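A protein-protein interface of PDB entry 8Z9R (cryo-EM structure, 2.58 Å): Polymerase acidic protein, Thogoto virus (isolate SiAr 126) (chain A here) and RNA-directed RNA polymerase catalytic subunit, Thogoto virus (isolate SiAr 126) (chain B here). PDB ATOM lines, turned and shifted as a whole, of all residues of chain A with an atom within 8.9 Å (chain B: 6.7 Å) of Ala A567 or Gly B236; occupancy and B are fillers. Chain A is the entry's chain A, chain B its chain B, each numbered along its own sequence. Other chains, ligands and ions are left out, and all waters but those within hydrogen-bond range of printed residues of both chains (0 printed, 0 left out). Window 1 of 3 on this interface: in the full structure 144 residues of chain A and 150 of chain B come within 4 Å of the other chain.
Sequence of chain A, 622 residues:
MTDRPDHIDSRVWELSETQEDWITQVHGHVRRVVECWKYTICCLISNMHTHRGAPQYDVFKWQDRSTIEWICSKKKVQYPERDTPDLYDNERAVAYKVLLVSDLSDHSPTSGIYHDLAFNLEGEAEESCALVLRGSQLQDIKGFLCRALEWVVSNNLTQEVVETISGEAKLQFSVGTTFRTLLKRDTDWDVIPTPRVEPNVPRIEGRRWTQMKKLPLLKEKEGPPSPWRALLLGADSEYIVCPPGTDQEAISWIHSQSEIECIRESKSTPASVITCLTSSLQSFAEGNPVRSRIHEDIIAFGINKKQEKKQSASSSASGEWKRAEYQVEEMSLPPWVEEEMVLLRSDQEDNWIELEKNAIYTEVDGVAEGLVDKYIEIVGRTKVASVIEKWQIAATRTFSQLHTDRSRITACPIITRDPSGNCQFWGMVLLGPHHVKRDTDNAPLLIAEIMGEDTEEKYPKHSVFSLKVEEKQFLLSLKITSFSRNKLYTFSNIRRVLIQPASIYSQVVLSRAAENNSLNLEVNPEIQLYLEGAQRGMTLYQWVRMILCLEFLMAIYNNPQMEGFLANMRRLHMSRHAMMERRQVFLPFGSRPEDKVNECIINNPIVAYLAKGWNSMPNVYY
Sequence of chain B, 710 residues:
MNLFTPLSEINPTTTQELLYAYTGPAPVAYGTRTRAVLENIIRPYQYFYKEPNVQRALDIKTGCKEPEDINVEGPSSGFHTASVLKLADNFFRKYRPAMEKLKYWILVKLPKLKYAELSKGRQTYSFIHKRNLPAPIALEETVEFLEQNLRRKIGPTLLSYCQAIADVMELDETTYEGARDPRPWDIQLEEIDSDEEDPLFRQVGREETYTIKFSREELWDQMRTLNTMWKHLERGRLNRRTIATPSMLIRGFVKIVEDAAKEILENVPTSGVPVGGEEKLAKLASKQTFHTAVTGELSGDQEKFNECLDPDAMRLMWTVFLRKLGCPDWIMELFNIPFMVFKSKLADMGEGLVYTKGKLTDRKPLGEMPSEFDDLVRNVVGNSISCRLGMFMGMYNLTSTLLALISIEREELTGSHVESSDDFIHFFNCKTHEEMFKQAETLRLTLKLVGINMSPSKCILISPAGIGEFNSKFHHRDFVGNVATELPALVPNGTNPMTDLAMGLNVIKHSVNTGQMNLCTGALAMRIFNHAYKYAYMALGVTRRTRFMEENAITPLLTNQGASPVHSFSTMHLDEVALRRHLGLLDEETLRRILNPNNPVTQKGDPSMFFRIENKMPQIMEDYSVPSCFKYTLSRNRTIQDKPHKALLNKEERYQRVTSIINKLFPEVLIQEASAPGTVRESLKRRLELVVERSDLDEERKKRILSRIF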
ATOM      1  N   ASN A 558      -8.275   9.400  -9.106  1.00  0.00           N
ATOM      2  CA  ASN A 558      -7.662  10.253 -10.114  1.00  0.00           C
ATOM      3  C   ASN A 558      -8.160   9.844 -11.495  1.00  0.00           C
ATOM      4  O   ASN A 558      -8.032   8.682 -11.892  1.00  0.00           O
ATOM      5  CB  ASN A 558      -6.141  10.158 -10.037  1.00  0.00           C
ATOM      6  CG  ASN A 558      -5.451  11.265 -10.800  1.00  0.00           C
ATOM      7  OD1 ASN A 558      -6.099  12.151 -11.351  1.00  0.00           O
ATOM      8  ND2 ASN A 558      -4.127  11.221 -10.838  1.00  0.00           N
ATOM      9  N   ASN A 559      -8.730  10.800 -12.219  1.00  0.00           N
ATOM     10  CA  ASN A 559      -9.252  10.588 -13.560  1.00  0.00           C
ATOM     11  C   ASN A 559      -9.090  11.890 -14.338  1.00  0.00           C
ATOM     12  O   ASN A 559      -8.596  12.874 -13.774  1.00  0.00           O
ATOM     13  CB  ASN A 559     -10.713  10.127 -13.503  1.00  0.00           C
ATOM     14  CG  ASN A 559     -11.564  10.980 -12.588  1.00  0.00           C
ATOM     15  OD1 ASN A 559     -11.368  12.189 -12.479  1.00  0.00           O
ATOM     16  ND2 ASN A 559     -12.526  10.351 -11.925  1.00  0.00           N
ATOM     17  N   PRO A 560      -9.452  11.937 -15.626  1.00  0.00           N
ATOM     18  CA  PRO A 560      -9.373  13.218 -16.350  1.00  0.00           C
ATOM     19  C   PRO A 560     -10.093  14.364 -15.658  1.00  0.00           C
ATOM     20  O   PRO A 560      -9.603  15.499 -15.684  1.00  0.00           O
ATOM     21  CB  PRO A 560     -10.017  12.891 -17.705  1.00  0.00           C
ATOM     22  CG  PRO A 560      -9.987  11.402 -17.832  1.00  0.00           C
ATOM     23  CD  PRO A 560      -9.510  10.795 -16.552  1.00  0.00           C
ATOM     24  N   GLN A 561     -11.245  14.098 -15.037  1.00  0.00           N
ATOM     25  CA  GLN A 561     -11.959  15.153 -14.328  1.00  0.00           C
ATOM     26  C   GLN A 561     -11.129  15.694 -13.170  1.00  0.00           C
ATOM     27  O   GLN A 561     -11.010  16.911 -12.993  1.00  0.00           O
ATOM     28  CB  GLN A 561     -13.308  14.634 -13.829  1.00  0.00           C
ATOM     29  CG  GLN A 561     -14.050  13.769 -14.829  1.00  0.00           C
ATOM     30  CD  GLN A 561     -15.387  13.297 -14.301  1.00  0.00           C
ATOM     31  OE1 GLN A 561     -15.958  13.904 -13.397  1.00  0.00           O
ATOM     32  NE2 GLN A 561     -15.893  12.205 -14.860  1.00  0.00           N
ATOM     33  N   MET A 562     -10.541  14.799 -12.372  1.00  0.00           N
ATOM     34  CA  MET A 562      -9.696  15.239 -11.266  1.00  0.00           C
ATOM     35  C   MET A 562      -8.473  15.991 -11.769  1.00  0.00           C
ATOM     36  O   MET A 562      -8.081  17.010 -11.190  1.00  0.00           O
ATOM     37  CB  MET A 562      -9.273  14.042 -10.415  1.00  0.00           C
ATOM     38  CG  MET A 562      -8.440  14.414  -9.198  1.00  0.00           C
ATOM     39  SD  MET A 562      -9.430  14.930  -7.784  1.00  0.00           S
ATOM     40  CE  MET A 562      -9.991  13.346  -7.172  1.00  0.00           C
ATOM     41  N   GLU A 563      -7.857  15.505 -12.849  1.00  0.00           N
ATOM     42  CA  GLU A 563      -6.678  16.167 -13.394  1.00  0.00           C
ATOM     43  C   GLU A 563      -7.003  17.589 -13.833  1.00  0.00           C
ATOM     44  O   GLU A 563      -6.304  18.541 -13.464  1.00  0.00           O
ATOM     45  CB  GLU A 563      -6.117  15.355 -14.560  1.00  0.00           C
ATOM     46  CG  GLU A 563      -5.543  14.008 -14.162  1.00  0.00           C
ATOM     47  CD  GLU A 563      -4.147  14.117 -13.586  1.00  0.00           C
ATOM     48  OE1 GLU A 563      -3.549  15.209 -13.677  1.00  0.00           O
ATOM     49  OE2 GLU A 563      -3.647  13.112 -13.040  1.00  0.00           O
ATOM     50  N   GLY A 564      -8.076  17.754 -14.609  1.00  0.00           N
ATOM     51  CA  GLY A 564      -8.458  19.084 -15.052  1.00  0.00           C
ATOM     52  C   GLY A 564      -8.860  19.991 -13.906  1.00  0.00           C
ATOM     53  O   GLY A 564      -8.480  21.166 -13.867  1.00  0.00           O
ATOM     54  N   PHE A 565      -9.626  19.457 -12.950  1.00  0.00           N
ATOM     55  CA  PHE A 565     -10.051  20.246 -11.801  1.00  0.00           C
ATOM     56  C   PHE A 565      -8.854  20.755 -11.011  1.00  0.00           C
ATOM     57  O   PHE A 565      -8.788  21.937 -10.656  1.00  0.00           O
ATOM     58  CB  PHE A 565     -10.967  19.403 -10.912  1.00  0.00           C
ATOM     59  CG  PHE A 565     -11.373  20.082  -9.638  1.00  0.00           C
ATOM     60  CD1 PHE A 565     -12.452  20.942  -9.611  1.00  0.00           C
ATOM     61  CD2 PHE A 565     -10.682  19.847  -8.461  1.00  0.00           C
ATOM     62  CE1 PHE A 565     -12.828  21.566  -8.442  1.00  0.00           C
ATOM     63  CE2 PHE A 565     -11.054  20.468  -7.289  1.00  0.00           C
ATOM     64  CZ  PHE A 565     -12.129  21.328  -7.280  1.00  0.00           C
ATOM     65  N   LEU A 566      -7.892  19.877 -10.730  1.00  0.00           N
ATOM     66  CA  LEU A 566      -6.741  20.284  -9.936  1.00  0.00           C
ATOM     67  C   LEU A 566      -5.833  21.222 -10.718  1.00  0.00           C
ATOM     68  O   LEU A 566      -5.218  22.122 -10.137  1.00  0.00           O
ATOM     69  CB  LEU A 566      -5.972  19.056  -9.463  1.00  0.00           C
ATOM     70  CG  LEU A 566      -6.681  18.272  -8.363  1.00  0.00           C
ATOM     71  CD1 LEU A 566      -5.841  17.097  -7.941  1.00  0.00           C
ATOM     72  CD2 LEU A 566      -6.994  19.168  -7.178  1.00  0.00           C
ATOM     73  N   ALA A 567      -5.732  21.029 -12.034  1.00  0.00           N
ATOM     74  CA  ALA A 567      -4.916  21.931 -12.838  1.00  0.00           C
ATOM     75  C   ALA A 567      -5.524  23.326 -12.891  1.00  0.00           C
ATOM     76  O   ALA A 567      -4.796  24.324 -12.923  1.00  0.00           O
ATOM     77  CB  ALA A 567      -4.744  21.367 -14.246  1.00  0.00           C
ATOM     78  N   ASN A 568      -6.851  23.417 -12.910  1.00  0.00           N
ATOM     79  CA  ASN A 568      -7.505  24.705 -13.068  1.00  0.00           C
ATOM     80  C   ASN A 568      -7.868  25.378 -11.748  1.00  0.00           C
ATOM     81  O   ASN A 568      -8.215  26.563 -11.758  1.00  0.00           O
ATOM     82  CB  ASN A 568      -8.750  24.542 -13.937  1.00  0.00           C
ATOM     83  CG  ASN A 568      -8.408  24.240 -15.380  1.00  0.00           C
ATOM     84  OD1 ASN A 568      -7.684  24.993 -16.027  1.00  0.00           O
ATOM     85  ND2 ASN A 568      -8.917  23.127 -15.887  1.00  0.00           N
ATOM     86  N   MET A 569      -7.799  24.670 -10.617  1.00  0.00           N
ATOM     87  CA  MET A 569      -7.954  25.337  -9.328  1.00  0.00           C
ATOM     88  C   MET A 569      -6.687  26.002  -8.822  1.00  0.00           C
ATOM     89  O   MET A 569      -6.759  26.728  -7.830  1.00  0.00           O
ATOM     90  CB  MET A 569      -8.447  24.374  -8.248  1.00  0.00           C
ATOM     91  CG  MET A 569      -9.843  23.853  -8.447  1.00  0.00           C
ATOM     92  SD  MET A 569     -10.969  25.257  -8.433  1.00  0.00           S
ATOM     93  CE  MET A 569     -10.857  25.746  -6.720  1.00  0.00           C
ATOM     94  N   ARG A 570      -5.536  25.775  -9.450  1.00  0.00           N
ATOM     95  CA  ARG A 570      -4.327  26.436  -8.973  1.00  0.00           C
ATOM     96  C   ARG A 570      -4.390  27.944  -9.194  1.00  0.00           C
ATOM     97  O   ARG A 570      -3.934  28.714  -8.340  1.00  0.00           O
ATOM     98  CB  ARG A 570      -3.103  25.818  -9.643  1.00  0.00           C
ATOM     99  CG  ARG A 570      -2.953  24.344  -9.308  1.00  0.00           C
ATOM    100  CD  ARG A 570      -1.640  23.761  -9.786  1.00  0.00           C
ATOM    101  NE  ARG A 570      -1.727  22.312  -9.924  1.00  0.00           N
ATOM    102  CZ  ARG A 570      -1.650  21.662 -11.076  1.00  0.00           C
ATOM    103  NH1 ARG A 570      -1.452  22.300 -12.216  1.00  0.00           N
ATOM    104  NH2 ARG A 570      -1.767  20.338 -11.083  1.00  0.00           N
ATOM    105  N   ARG A 571      -4.972  28.382 -10.312  1.00  0.00           N
ATOM    106  CA  ARG A 571      -5.162  29.811 -10.541  1.00  0.00           C
ATOM    107  C   ARG A 571      -6.068  30.430  -9.484  1.00  0.00           C
ATOM    108  O   ARG A 571      -5.775  31.509  -8.961  1.00  0.00           O
ATOM    109  CB  ARG A 571      -5.742  30.044 -11.934  1.00  0.00           C
ATOM    110  CG  ARG A 571      -4.724  30.475 -12.965  1.00  0.00           C
ATOM    111  CD  ARG A 571      -5.356  30.594 -14.335  1.00  0.00           C
ATOM    112  NE  ARG A 571      -6.347  29.553 -14.571  1.00  0.00           N
ATOM    113  CZ  ARG A 571      -6.077  28.378 -15.120  1.00  0.00           C
ATOM    114  NH1 ARG A 571      -4.851  28.054 -15.494  1.00  0.00           N
ATOM    115  NH2 ARG A 571      -7.062  27.503 -15.299  1.00  0.00           N
ATOM    116  N   LEU A 572      -7.174  29.757  -9.152  1.00  0.00           N
ATOM    117  CA  LEU A 572      -8.089  30.289  -8.150  1.00  0.00           C
ATOM    118  C   LEU A 572      -7.479  30.253  -6.755  1.00  0.00           C
ATOM    119  O   LEU A 572      -7.730  31.151  -5.947  1.00  0.00           O
ATOM    120  CB  LEU A 572      -9.404  29.514  -8.181  1.00  0.00           C
ATOM    121  CG  LEU A 572     -10.227  29.683  -9.458  1.00  0.00           C
ATOM    122  CD1 LEU A 572     -11.459  28.799  -9.426  1.00  0.00           C
ATOM    123  CD2 LEU A 572     -10.610  31.136  -9.656  1.00  0.00           C
ATOM    124  N   HIS A 573      -6.684  29.225  -6.457  1.00  0.00           N
ATOM    125  CA  HIS A 573      -5.965  29.158  -5.191  1.00  0.00           C
ATOM    126  C   HIS A 573      -4.988  30.321  -5.062  1.00  0.00           C
ATOM    127  O   HIS A 573      -4.907  30.966  -4.008  1.00  0.00           O
ATOM    128  CB  HIS A 573      -5.243  27.813  -5.107  1.00  0.00           C
ATOM    129  CG  HIS A 573      -5.008  27.321  -3.714  1.00  0.00           C
ATOM    130  ND1 HIS A 573      -5.919  26.536  -3.041  1.00  0.00           N
ATOM    131  CD2 HIS A 573      -3.942  27.448  -2.890  1.00  0.00           C
ATOM    132  CE1 HIS A 573      -5.440  26.231  -1.850  1.00  0.00           C
ATOM    133  NE2 HIS A 573      -4.241  26.769  -1.734  1.00  0.00           N
ATOM    134  N   PRO A 593     -12.633  32.528 -15.003  1.00  0.00           N
ATOM    135  CA  PRO A 593     -11.747  31.413 -14.631  1.00  0.00           C
ATOM    136  C   PRO A 593     -12.478  30.205 -14.077  1.00  0.00           C
ATOM    137  O   PRO A 593     -11.902  29.111 -14.054  1.00  0.00           O
ATOM    138  CB  PRO A 593     -10.823  32.038 -13.579  1.00  0.00           C
ATOM    139  CG  PRO A 593     -10.880  33.506 -13.851  1.00  0.00           C
ATOM    140  CD  PRO A 593     -12.291  33.761 -14.276  1.00  0.00           C
ATOM    141  N   LYS A 596     -13.494  26.864 -16.674  1.00  0.00           N
ATOM    142  CA  LYS A 596     -12.543  25.795 -16.937  1.00  0.00           C
ATOM    143  C   LYS A 596     -12.400  24.843 -15.758  1.00  0.00           C
ATOM    144  O   LYS A 596     -11.807  23.771 -15.917  1.00  0.00           O
ATOM    145  CB  LYS A 596     -11.192  26.397 -17.326  1.00  0.00           C
ATOM    146  CG  LYS A 596     -11.244  27.150 -18.650  1.00  0.00           C
ATOM    147  CD  LYS A 596      -9.893  27.695 -19.051  1.00  0.00           C
ATOM    148  CE  LYS A 596      -9.987  28.493 -20.338  1.00  0.00           C
ATOM    149  NZ  LYS A 596     -10.340  27.642 -21.506  1.00  0.00           N
ATOM    150  N   VAL A 597     -12.923  25.210 -14.591  1.00  0.00           N
ATOM    151  CA  VAL A 597     -13.051  24.276 -13.479  1.00  0.00           C
ATOM    152  C   VAL A 597     -14.393  23.556 -13.527  1.00  0.00           C
ATOM    153  O   VAL A 597     -14.460  22.343 -13.316  1.00  0.00           O
ATOM    154  CB  VAL A 597     -12.865  25.019 -12.139  1.00  0.00           C
ATOM    155  CG1 VAL A 597     -13.010  24.060 -10.986  1.00  0.00           C
ATOM    156  CG2 VAL A 597     -11.525  25.710 -12.081  1.00  0.00           C
ATOM    157  N   GLU A 599     -16.222  22.810 -16.031  1.00  0.00           N
ATOM    158  CA  GLU A 599     -16.270  21.791 -17.070  1.00  0.00           C
ATOM    159  C   GLU A 599     -15.684  20.463 -16.606  1.00  0.00           C
ATOM    160  O   GLU A 599     -15.985  19.426 -17.205  1.00  0.00           O
ATOM    161  CB  GLU A 599     -15.548  22.289 -18.321  1.00  0.00           C
ATOM    162  CG  GLU A 599     -14.104  22.676 -18.087  1.00  0.00           C
ATOM    163  CD  GLU A 599     -13.334  22.840 -19.379  1.00  0.00           C
ATOM    164  OE1 GLU A 599     -13.770  23.636 -20.236  1.00  0.00           O
ATOM    165  OE2 GLU A 599     -12.290  22.176 -19.536  1.00  0.00           O
ATOM    166  N   CYS A 600     -14.868  20.469 -15.555  1.00  0.00           N
ATOM    167  CA  CYS A 600     -14.270  19.255 -15.016  1.00  0.00           C
ATOM    168  C   CYS A 600     -15.056  18.661 -13.853  1.00  0.00           C
ATOM    169  O   CYS A 600     -14.655  17.620 -13.324  1.00  0.00           O
ATOM    170  CB  CYS A 600     -12.831  19.529 -14.568  1.00  0.00           C
ATOM    171  SG  CYS A 600     -11.844  20.453 -15.762  1.00  0.00           S
ATOM    172  N   LEU B  19      -2.419  20.394  -4.429  1.00  0.00           N
ATOM    173  CA  LEU B  19      -3.329  20.357  -5.575  1.00  0.00           C
ATOM    174  C   LEU B  19      -2.762  19.502  -6.702  1.00  0.00           C
ATOM    175  O   LEU B  19      -2.698  19.915  -7.858  1.00  0.00           O
ATOM    176  CB  LEU B  19      -3.616  21.773  -6.055  1.00  0.00           C
ATOM    177  CG  LEU B  19      -4.120  22.759  -5.002  1.00  0.00           C
ATOM    178  CD1 LEU B  19      -4.473  24.088  -5.641  1.00  0.00           C
ATOM    179  CD2 LEU B  19      -5.311  22.184  -4.265  1.00  0.00           C
ATOM    180  N   TYR B  22      -1.181  13.296  -8.323  1.00  0.00           N
ATOM    181  CA  TYR B  22      -0.199  12.346  -8.813  1.00  0.00           C
ATOM    182  C   TYR B  22      -0.027  11.222  -7.794  1.00  0.00           C
ATOM    183  O   TYR B  22      -0.508  11.299  -6.659  1.00  0.00           O
ATOM    184  CB  TYR B  22       1.134  13.037  -9.104  1.00  0.00           C
ATOM    185  CG  TYR B  22       1.067  14.131 -10.156  1.00  0.00           C
ATOM    186  CD1 TYR B  22      -0.084  14.348 -10.901  1.00  0.00           C
ATOM    187  CD2 TYR B  22       2.168  14.929 -10.421  1.00  0.00           C
ATOM    188  CE1 TYR B  22      -0.142  15.344 -11.854  1.00  0.00           C
ATOM    189  CE2 TYR B  22       2.122  15.923 -11.375  1.00  0.00           C
ATOM    190  CZ  TYR B  22       0.966  16.125 -12.089  1.00  0.00           C
ATOM    191  OH  TYR B  22       0.916  17.115 -13.042  1.00  0.00           O
ATOM    192  N   PRO B  27      -4.517   9.680 -17.086  1.00  0.00           N
ATOM    193  CA  PRO B  27      -5.539   9.377 -18.092  1.00  0.00           C
ATOM    194  C   PRO B  27      -4.927   8.938 -19.412  1.00  0.00           C
ATOM    195  O   PRO B  27      -3.822   9.342 -19.780  1.00  0.00           O
ATOM    196  CB  PRO B  27      -6.294  10.702 -18.243  1.00  0.00           C
ATOM    197  CG  PRO B  27      -5.340  11.738 -17.775  1.00  0.00           C
ATOM    198  CD  PRO B  27      -4.531  11.098 -16.693  1.00  0.00           C
ATOM    199  N   GLU B 234      -0.924  11.769 -20.198  1.00  0.00           N
ATOM    200  CA  GLU B 234      -0.760  13.205 -20.021  1.00  0.00           C
ATOM    201  C   GLU B 234      -1.641  13.678 -18.874  1.00  0.00           C
ATOM    202  O   GLU B 234      -2.841  13.393 -18.848  1.00  0.00           O
ATOM    203  CB  GLU B 234      -1.104  13.968 -21.298  1.00  0.00           C
ATOM    204  CG  GLU B 234      -0.868  15.464 -21.186  1.00  0.00           C
ATOM    205  CD  GLU B 234      -1.166  16.196 -22.473  1.00  0.00           C
ATOM    206  OE1 GLU B 234      -1.579  15.533 -23.446  1.00  0.00           O
ATOM    207  OE2 GLU B 234      -0.985  17.430 -22.515  1.00  0.00           O
ATOM    208  N   ARG B 235      -1.044  14.407 -17.938  1.00  0.00           N
ATOM    209  CA  ARG B 235      -1.723  14.855 -16.735  1.00  0.00           C
ATOM    210  C   ARG B 235      -2.013  16.347 -16.813  1.00  0.00           C
ATOM    211  O   ARG B 235      -1.269  17.110 -17.434  1.00  0.00           O
ATOM    212  CB  ARG B 235      -0.882  14.555 -15.492  1.00  0.00           C
ATOM    213  CG  ARG B 235      -0.105  13.255 -15.577  1.00  0.00           C
ATOM    214  CD  ARG B 235       0.573  12.934 -14.262  1.00  0.00           C
ATOM    215  NE  ARG B 235      -0.343  12.297 -13.326  1.00  0.00           N
ATOM    216  CZ  ARG B 235      -0.192  11.069 -12.852  1.00  0.00           C
ATOM    217  NH1 ARG B 235       0.844  10.321 -13.189  1.00  0.00           N
ATOM    218  NH2 ARG B 235      -1.104  10.581 -12.015  1.00  0.00           N
ATOM    219  N   GLY B 236      -3.108  16.753 -16.180  1.00  0.00           N
ATOM    220  CA  GLY B 236      -3.473  18.149 -16.095  1.00  0.00           C
ATOM    221  C   GLY B 236      -4.503  18.629 -17.093  1.00  0.00           C
ATOM    222  O   GLY B 236      -4.753  19.837 -17.158  1.00  0.00           O
ATOM    223  N   ARG B 237      -5.104  17.734 -17.870  1.00  0.00           N
ATOM    224  CA  ARG B 237      -6.088  18.118 -18.870  1.00  0.00           C
ATOM    225  C   ARG B 237      -7.294  17.197 -18.793  1.00  0.00           C
ATOM    226  O   ARG B 237      -7.151  15.984 -18.610  1.00  0.00           O
ATOM    227  CB  ARG B 237      -5.489  18.081 -20.282  1.00  0.00           C
ATOM    228  CG  ARG B 237      -4.468  19.172 -20.548  1.00  0.00           C
ATOM    229  CD  ARG B 237      -3.860  19.036 -21.930  1.00  0.00           C
ATOM    230  NE  ARG B 237      -4.854  18.644 -22.920  1.00  0.00           N
ATOM    231  CZ  ARG B 237      -5.551  19.497 -23.659  1.00  0.00           C
ATOM    232  NH1 ARG B 237      -5.384  20.804 -23.547  1.00  0.00           N
ATOM    233  NH2 ARG B 237      -6.437  19.027 -24.532  1.00  0.00           N
ATOM    234  N   LEU B 238      -8.486  17.784 -18.926  1.00  0.00           N
ATOM    235  CA  LEU B 238      -9.708  16.989 -18.937  1.00  0.00           C
ATOM    236  C   LEU B 238      -9.881  16.254 -20.260  1.00  0.00           C
ATOM    237  O   LEU B 238     -10.277  15.082 -20.279  1.00  0.00           O
ATOM    238  CB  LEU B 238     -10.915  17.885 -18.665  1.00  0.00           C
ATOM    239  CG  LEU B 238     -12.298  17.266 -18.878  1.00  0.00           C
ATOM    240  CD1 LEU B 238     -12.608  16.239 -17.806  1.00  0.00           C
ATOM    241  CD2 LEU B 238     -13.365  18.345 -18.916  1.00  0.00           C
ATOM    242  N   ARG B 240      -8.505  14.719 -23.917  1.00  0.00           N
ATOM    243  CA  ARG B 240      -7.319  14.194 -24.579  1.00  0.00           C
ATOM    244  C   ARG B 240      -6.995  15.021 -25.816  1.00  0.00           C
ATOM    245  O   ARG B 240      -7.889  15.452 -26.549  1.00  0.00           O
ATOM    246  CB  ARG B 240      -7.531  12.732 -24.970  1.00  0.00           C
ATOM    247  CG  ARG B 240      -8.124  11.860 -23.877  1.00  0.00           C
ATOM    248  CD  ARG B 240      -7.070  11.385 -22.886  1.00  0.00           C
ATOM    249  NE  ARG B 240      -6.677  12.424 -21.942  1.00  0.00           N
ATOM    250  CZ  ARG B 240      -7.441  12.871 -20.955  1.00  0.00           C
ATOM    251  NH1 ARG B 240      -8.656  12.390 -20.750  1.00  0.00           N
ATOM    252  NH2 ARG B 240      -6.975  13.824 -20.154  1.00  0.00           N
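ND2 of Asn A558 lies close to NH2 of Arg B235 (3.3 Å).
The guanidinium group of Arg B235 is in salt-bridge range of the side-chain carboxylate of Glu A563 (3.4 Å).
The backbone NH of Gly B236 sits at hydrogen-bond distance from the side-chain carboxylate of Glu A563, 3.0 Å away.
The guanidinium group (NE) of Arg A570 lies within hydrogen-bond range of the backbone carbonyl oxygen (O) of Leu B19.
O of Arg B237 lies within hydrogen-bond range of NH2 of Arg B240 (2.7 Å).
N of Gln A561 sits close to OD1 of Asn A559.
NH1 of Arg B240 is in hydrogen-bond range of O of Leu B238 (3.2 Å).
The side-chain amide nitrogen (ND2) of Asn A558 lies within hydrogen-bond range of the side-chain carboxylate (OE2) of Glu A563 (2.9 Å).
O of Lys A596 sits at hydrogen-bond distance from SG of Cys A600 (3.3 Å).
The backbone NH (N) of Phe A565 sits close to the side-chain sulfur (SG) of Cys A600 (3.7 Å).
Ala A567 touches just one residue of chain B: Gly B236 (3.3 Å).
Gly B236 touches just these residues of chain A: Glu A563 (3.0 Å) and Ala A567 (3.3 Å).
Printed residues of chain B within 4 Å of Glu A563: Tyr B22, Pro B27, Arg B235 and Gly B236.
Of the printed residues of chain A, Pro B27 touches Pro A560 and Glu A563.
Of the printed residues of chain A, Leu B19 touches Leu A566 (3.7 Å), Arg A570 (3.3 Å) and His A573 (3.8 Å).
Met A562 touches none of the printed residues of chain B.
Phe A565 touches none of the printed residues of chain B.
Among the printed residues, merely in contact across the chains: Ala A567 with Gly B236 (3.3 Å), Glu A599 with Leu B238 (3.3 Å), Pro A560 with Arg B240 (3.4 Å), Pro A560 with Leu B238 (3.4 Å), Pro A560 with Pro B27 (3.6 Å), Gln A561 with Leu B238 (3.7 Å), Leu A566 with Leu B19 (3.7 Å), His A573 with Leu B19 (3.8 Å), Pro A560 with Arg B237 (3.8 Å), Glu A563 with Tyr B22 (3.9 Å), Cys A600 with Leu B238 (3.99 Å) and Glu A563 with Pro B27 (3.99 Å).
Of the 9 printed residues of chain B, 8 touch a printed residue of chain A.
Hydrophobic or aromatic side chains of chain B that line the printed part of chain A: Leu B19, Tyr B22, Pro B27 and Leu B238.
Among the printed residues, Asp or Glu carboxylates within 4 Å of a Lys or Arg side-chain nitrogen of the other chain: Glu A563 with Arg B235 (3.4 Å).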
